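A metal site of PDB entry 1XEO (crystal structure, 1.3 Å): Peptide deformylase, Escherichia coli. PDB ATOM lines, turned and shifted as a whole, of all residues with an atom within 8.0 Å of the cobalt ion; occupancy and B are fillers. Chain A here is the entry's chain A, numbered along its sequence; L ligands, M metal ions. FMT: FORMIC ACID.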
ATOM      1  N   VAL A   5       5.730  -2.726 -13.460  1.00  0.00           N
ATOM      2  CA  VAL A   5       5.159  -2.890 -12.124  1.00  0.00           C
ATOM      3  C   VAL A   5       3.928  -2.028 -11.995  1.00  0.00           C
ATOM      4  O   VAL A   5       3.980  -0.794 -12.288  1.00  0.00           O
ATOM      5  CB  VAL A   5       6.191  -2.506 -11.033  1.00  0.00           C
ATOM      6  CG1 VAL A   5       5.585  -2.654  -9.659  1.00  0.00           C
ATOM      7  CG2 VAL A   5       7.438  -3.415 -11.183  1.00  0.00           C
ATOM      8  N   LEU A  13      -4.089  -4.973  -8.694  1.00  0.00           N
ATOM      9  CA  LEU A  13      -3.316  -5.266  -7.471  1.00  0.00           C
ATOM     10  C   LEU A  13      -4.164  -5.908  -6.428  1.00  0.00           C
ATOM     11  O   LEU A  13      -3.627  -6.361  -5.403  1.00  0.00           O
ATOM     12  CB  LEU A  13      -2.689  -3.974  -6.953  1.00  0.00           C
ATOM     13  CG  LEU A  13      -1.537  -3.443  -7.763  1.00  0.00           C
ATOM     14  CD1 LEU A  13      -1.203  -2.021  -7.337  1.00  0.00           C
ATOM     15  CD2 LEU A  13      -0.306  -4.323  -7.559  1.00  0.00           C
ATOM     16  N   GLY A  45      11.824  -7.428  -2.719  1.00  0.00           N
ATOM     17  CA  GLY A  45      10.849  -8.497  -2.959  1.00  0.00           C
ATOM     18  C   GLY A  45       9.931  -8.073  -4.061  1.00  0.00           C
ATOM     19  O   GLY A  45       9.790  -6.869  -4.328  1.00  0.00           O
ATOM     20  N   LEU A  46       9.276  -9.036  -4.694  1.00  0.00           N
ATOM     21  CA  LEU A  46       8.290  -8.776  -5.736  1.00  0.00           C
ATOM     22  C   LEU A  46       7.334  -9.940  -5.818  1.00  0.00           C
ATOM     23  O   LEU A  46       7.796 -11.106  -5.842  1.00  0.00           O
ATOM     24  CB  LEU A  46       9.006  -8.518  -7.079  1.00  0.00           C
ATOM     25  CG  LEU A  46       8.099  -8.095  -8.255  1.00  0.00           C
ATOM     26  CD1 LEU A  46       7.579  -6.675  -8.060  1.00  0.00           C
ATOM     27  CD2 LEU A  46       8.903  -8.188  -9.562  1.00  0.00           C
ATOM     28  N   ALA A  47       6.066  -9.664  -5.869  1.00  0.00           N
ATOM     29  CA  ALA A  47       5.036 -10.731  -6.007  1.00  0.00           C
ATOM     30  C   ALA A  47       4.517 -10.663  -7.443  1.00  0.00           C
ATOM     31  O   ALA A  47       4.422  -9.541  -8.054  1.00  0.00           O
ATOM     32  CB  ALA A  47       3.913 -10.477  -5.037  1.00  0.00           C
ATOM     33  N   GLN A  50       2.031  -8.030  -8.733  1.00  0.00           N
ATOM     34  CA  GLN A  50       2.495  -6.687  -9.036  1.00  0.00           C
ATOM     35  C   GLN A  50       2.885  -6.488 -10.470  1.00  0.00           C
ATOM     36  O   GLN A  50       3.051  -5.317 -10.881  1.00  0.00           O
ATOM     37  CB  GLN A  50       3.673  -6.347  -8.124  1.00  0.00           C
ATOM     38  CG  GLN A  50       3.336  -6.241  -6.638  1.00  0.00           C
ATOM     39  CD  GLN A  50       4.545  -5.946  -5.863  1.00  0.00           C
ATOM     40  OE1 GLN A  50       5.279  -6.853  -5.420  1.00  0.00           O
ATOM     41  NE2 GLN A  50       4.831  -4.629  -5.705  1.00  0.00           N
ATOM     42  N   GLU A  88       7.681   0.219   6.068  1.00  0.00           N
ATOM     43  CA  GLU A  88       7.745  -0.489   4.803  1.00  0.00           C
ATOM     44  C   GLU A  88       7.487   0.392   3.616  1.00  0.00           C
ATOM     45  O   GLU A  88       6.677   1.322   3.695  1.00  0.00           O
ATOM     46  CB  GLU A  88       6.657  -1.614   4.809  1.00  0.00           C
ATOM     47  CG  GLU A  88       6.929  -2.726   5.844  1.00  0.00           C
ATOM     48  CD  GLU A  88       5.922  -3.862   5.760  1.00  0.00           C
ATOM     49  OE1 GLU A  88       5.298  -4.128   4.669  1.00  0.00           O
ATOM     50  OE2 GLU A  88       5.722  -4.534   6.780  1.00  0.00           O
ATOM     51  N   GLY A  89       8.149   0.052   2.536  1.00  0.00           N
ATOM     52  CA  GLY A  89       7.817   0.639   1.245  1.00  0.00           C
ATOM     53  C   GLY A  89       7.272  -0.476   0.367  1.00  0.00           C
ATOM     54  O   GLY A  89       7.119  -1.633   0.803  1.00  0.00           O
ATOM     55  N   CYS A  90       6.996  -0.135  -0.877  1.00  0.00           N
ATOM     56  CA  CYS A  90       6.412  -1.102  -1.829  1.00  0.00           C
ATOM     57  C   CYS A  90       6.680  -0.553  -3.223  1.00  0.00           C
ATOM     58  O   CYS A  90       6.388   0.636  -3.477  1.00  0.00           O
ATOM     59  CB  CYS A  90       4.868  -1.198  -1.580  1.00  0.00           C
ATOM     60  SG  CYS A  90       4.002  -2.406  -2.599  1.00  0.00           S
ATOM     61  N   LEU A  91       7.106  -1.393  -4.164  1.00  0.00           N
ATOM     62  CA  LEU A  91       7.284  -0.960  -5.544  1.00  0.00           C
ATOM     63  C   LEU A  91       5.964  -0.527  -6.204  1.00  0.00           C
ATOM     64  O   LEU A  91       6.008   0.210  -7.202  1.00  0.00           O
ATOM     65  CB  LEU A  91       7.910  -2.081  -6.370  1.00  0.00           C
ATOM     66  CG  LEU A  91       9.298  -2.484  -5.896  1.00  0.00           C
ATOM     67  CD1 LEU A  91       9.734  -3.696  -6.742  1.00  0.00           C
ATOM     68  CD2 LEU A  91      10.296  -1.334  -6.064  1.00  0.00           C
ATOM     69  N   SER A  92       4.830  -0.937  -5.677  1.00  0.00           N
ATOM     70  CA  SER A  92       3.555  -0.556  -6.215  1.00  0.00           C
ATOM     71  C   SER A  92       2.974   0.735  -5.578  1.00  0.00           C
ATOM     72  O   SER A  92       1.902   1.206  -6.017  1.00  0.00           O
ATOM     73  CB  SER A  92       2.547  -1.683  -6.051  1.00  0.00           C
ATOM     74  OG  SER A  92       2.903  -2.752  -6.937  1.00  0.00           O
ATOM     75  N   ILE A  93       3.665   1.252  -4.534  1.00  0.00           N
ATOM     76  CA  ILE A  93       3.228   2.494  -3.828  1.00  0.00           C
ATOM     77  C   ILE A  93       4.515   3.310  -3.787  1.00  0.00           C
ATOM     78  O   ILE A  93       5.092   3.564  -2.721  1.00  0.00           O
ATOM     79  CB  ILE A  93       2.724   2.147  -2.445  1.00  0.00           C
ATOM     80  CG1 ILE A  93       1.629   1.036  -2.537  1.00  0.00           C
ATOM     81  CG2 ILE A  93       2.136   3.402  -1.811  1.00  0.00           C
ATOM     82  CD1 ILE A  93       1.029   0.649  -1.180  1.00  0.00           C
ATOM     83  N   ARG A 102       3.461  -6.621  11.927  1.00  0.00           N
ATOM     84  CA  ARG A 102       3.811  -7.902  11.291  1.00  0.00           C
ATOM     85  C   ARG A 102       4.188  -8.870  12.406  1.00  0.00           C
ATOM     86  O   ARG A 102       4.573  -8.472  13.505  1.00  0.00           O
ATOM     87  CB  ARG A 102       5.080  -7.757  10.420  1.00  0.00           C
ATOM     88  CG  ARG A 102       4.885  -6.816   9.202  1.00  0.00           C
ATOM     89  CD  ARG A 102       3.956  -7.426   8.205  1.00  0.00           C
ATOM     90  NE  ARG A 102       3.942  -6.594   6.988  1.00  0.00           N
ATOM     91  CZ  ARG A 102       3.053  -6.750   6.004  1.00  0.00           C
ATOM     92  NH1 ARG A 102       2.112  -7.690   6.046  1.00  0.00           N
ATOM     93  NH2 ARG A 102       3.140  -5.922   4.967  1.00  0.00           N
ATOM     94  N   CYS A 129       9.474  -9.199   5.026  1.00  0.00           N
ATOM     95  CA  CYS A 129       9.342  -9.205   3.567  1.00  0.00           C
ATOM     96  C   CYS A 129       8.462 -10.345   3.095  1.00  0.00           C
ATOM     97  O   CYS A 129       7.607 -10.148   2.252  1.00  0.00           O
ATOM     98  CB  CYS A 129      10.742  -9.335   3.004  1.00  0.00           C
ATOM     99  SG  CYS A 129      10.918  -9.351   1.269  1.00  0.00           S
ATOM    100  N   HIS A 132       4.867  -9.342   3.627  1.00  0.00           N
ATOM    101  CA  HIS A 132       4.474  -8.329   2.657  1.00  0.00           C
ATOM    102  C   HIS A 132       4.180  -8.978   1.310  1.00  0.00           C
ATOM    103  O   HIS A 132       3.169  -8.660   0.694  1.00  0.00           O
ATOM    104  CB  HIS A 132       5.621  -7.324   2.606  1.00  0.00           C
ATOM    105  CG  HIS A 132       5.414  -6.207   1.643  1.00  0.00           C
ATOM    106  ND1 HIS A 132       5.299  -4.881   2.017  1.00  0.00           N
ATOM    107  CD2 HIS A 132       5.373  -6.208   0.291  1.00  0.00           C
ATOM    108  CE1 HIS A 132       5.177  -4.143   0.868  1.00  0.00           C
ATOM    109  NE2 HIS A 132       5.222  -4.893  -0.247  1.00  0.00           N
ATOM    110  N   GLU A 133       5.081  -9.813   0.846  1.00  0.00           N
ATOM    111  CA  GLU A 133       4.867 -10.425  -0.461  1.00  0.00           C
ATOM    112  C   GLU A 133       3.727 -11.393  -0.460  1.00  0.00           C
ATOM    113  O   GLU A 133       2.953 -11.426  -1.431  1.00  0.00           O
ATOM    114  CB  GLU A 133       6.124 -11.124  -0.948  1.00  0.00           C
ATOM    115  CG  GLU A 133       7.389 -10.213  -0.994  1.00  0.00           C
ATOM    116  CD  GLU A 133       7.201  -8.946  -1.723  1.00  0.00           C
ATOM    117  OE1 GLU A 133       6.367  -8.876  -2.593  1.00  0.00           O
ATOM    118  OE2 GLU A 133       7.992  -8.028  -1.365  1.00  0.00           O
ATOM    119  N   ASP A 135       1.075 -11.116   1.274  1.00  0.00           N
ATOM    120  CA  ASP A 135      -0.131 -10.300   1.254  1.00  0.00           C
ATOM    121  C   ASP A 135      -0.431  -9.869  -0.208  1.00  0.00           C
ATOM    122  O   ASP A 135      -1.611  -9.885  -0.573  1.00  0.00           O
ATOM    123  CB  ASP A 135       0.031  -9.009   2.095  1.00  0.00           C
ATOM    124  CG  ASP A 135      -0.295  -9.160   3.531  1.00  0.00           C
ATOM    125  OD1 ASP A 135      -0.745 -10.232   3.987  1.00  0.00           O
ATOM    126  OD2 ASP A 135      -0.149  -8.146   4.296  1.00  0.00           O
ATOM    127  N   HIS A 136       0.596  -9.542  -0.994  1.00  0.00           N
ATOM    128  CA  HIS A 136       0.269  -9.129  -2.381  1.00  0.00           C
ATOM    129  C   HIS A 136      -0.494 -10.232  -3.132  1.00  0.00           C
ATOM    130  O   HIS A 136      -1.388  -9.946  -3.922  1.00  0.00           O
ATOM    131  CB  HIS A 136       1.554  -8.887  -3.178  1.00  0.00           C
ATOM    132  CG  HIS A 136       2.143  -7.511  -3.034  1.00  0.00           C
ATOM    133  ND1 HIS A 136       1.447  -6.364  -3.385  1.00  0.00           N
ATOM    134  CD2 HIS A 136       3.363  -7.103  -2.631  1.00  0.00           C
ATOM    135  CE1 HIS A 136       2.272  -5.304  -3.156  1.00  0.00           C
ATOM    136  NE2 HIS A 136       3.453  -5.689  -2.707  1.00  0.00           N
ATOM    137  N   LYS A 140      -3.663  -7.834  -1.044  1.00  0.00           N
ATOM    138  CA  LYS A 140      -3.541  -6.986   0.133  1.00  0.00           C
ATOM    139  C   LYS A 140      -2.258  -6.183   0.021  1.00  0.00           C
ATOM    140  O   LYS A 140      -1.198  -6.686  -0.339  1.00  0.00           O
ATOM    141  CB  LYS A 140      -3.580  -7.835   1.389  1.00  0.00           C
ATOM    142  CG  LYS A 140      -3.496  -7.034   2.701  1.00  0.00           C
ATOM    143  CD  LYS A 140      -3.795  -7.953   3.921  1.00  0.00           C
ATOM    144  CE  LYS A 140      -4.161  -7.124   5.129  1.00  0.00           C
ATOM    145  NZ  LYS A 140      -4.322  -8.044   6.311  1.00  0.00           N
ATOM    146  N   LEU A 141      -2.372  -4.883   0.357  1.00  0.00           N
ATOM    147  CA  LEU A 141      -1.248  -3.942   0.280  1.00  0.00           C
ATOM    148  C   LEU A 141      -0.940  -3.433   1.688  1.00  0.00           C
ATOM    149  O   LEU A 141      -1.832  -3.420   2.549  1.00  0.00           O
ATOM    150  CB  LEU A 141      -1.635  -2.742  -0.598  1.00  0.00           C
ATOM    151  CG  LEU A 141      -1.996  -3.104  -2.035  1.00  0.00           C
ATOM    152  CD1 LEU A 141      -2.541  -1.832  -2.746  1.00  0.00           C
ATOM    153  CD2 LEU A 141      -0.782  -3.677  -2.771  1.00  0.00           C
ATOM    154  N   PHE A 142       0.278  -2.933   1.926  1.00  0.00           N
ATOM    155  CA  PHE A 142       0.612  -2.540   3.288  1.00  0.00           C
ATOM    156  C   PHE A 142      -0.242  -1.378   3.781  1.00  0.00           C
ATOM    157  O   PHE A 142      -0.504  -1.228   4.991  1.00  0.00           O
ATOM    158  CB  PHE A 142       2.124  -2.237   3.441  1.00  0.00           C
ATOM    159  CG  PHE A 142       2.573  -0.872   2.967  1.00  0.00           C
ATOM    160  CD1 PHE A 142       2.290   0.295   3.701  1.00  0.00           C
ATOM    161  CD2 PHE A 142       3.272  -0.712   1.775  1.00  0.00           C
ATOM    162  CE1 PHE A 142       2.703   1.578   3.230  1.00  0.00           C
ATOM    163  CE2 PHE A 142       3.699   0.607   1.320  1.00  0.00           C
ATOM    164  CZ  PHE A 142       3.408   1.709   2.037  1.00  0.00           C
HETATM  165  C   FMT L   1       7.471  -5.385  -3.142  1.00  0.00           C
HETATM  166  O1  FMT L   1       6.387  -6.173  -2.833  1.00  0.00           O
HETATM  167  O2  FMT L   1       6.792  -4.158  -3.536  1.00  0.00           O
HETATM  168 CO    CO M   1       4.957  -4.461  -2.182  1.00  0.00          CO
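Gln 50 touches the cobalt ion.
The cobalt ion is bound by NE2 of His 132 (2.0 Å). NE2 of His 136 is bound to the cobalt ion. O2 of the ligand binds the cobalt ion. SG of Cys 90 is bound to the cobalt ion (2.3 Å). The cobalt ion is bound by O1 of the ligand (2.3 Å).
A ring nitrogen (ND1) of His 132 lies within hydrogen-bond range of the side-chain carboxylate (OE1) of Glu 88, 2.8 Å away. The side-chain amide nitrogen (NE2) of Gln 50 sits close to a ring nitrogen (NE2) of His 136 (3.5 Å). The side-chain sulfur (SG) of Cys 90 lies close to the backbone NH (N) of Ser 92. The side-chain hydroxyl (OG) of Ser 92 is in hydrogen-bond range of the side-chain amide nitrogen (NE2) of Gln 50. The backbone NH (N) of Ala 47 sits at hydrogen-bond distance from the side-chain amide oxygen (OE1) of Gln 50 (3.0 Å).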
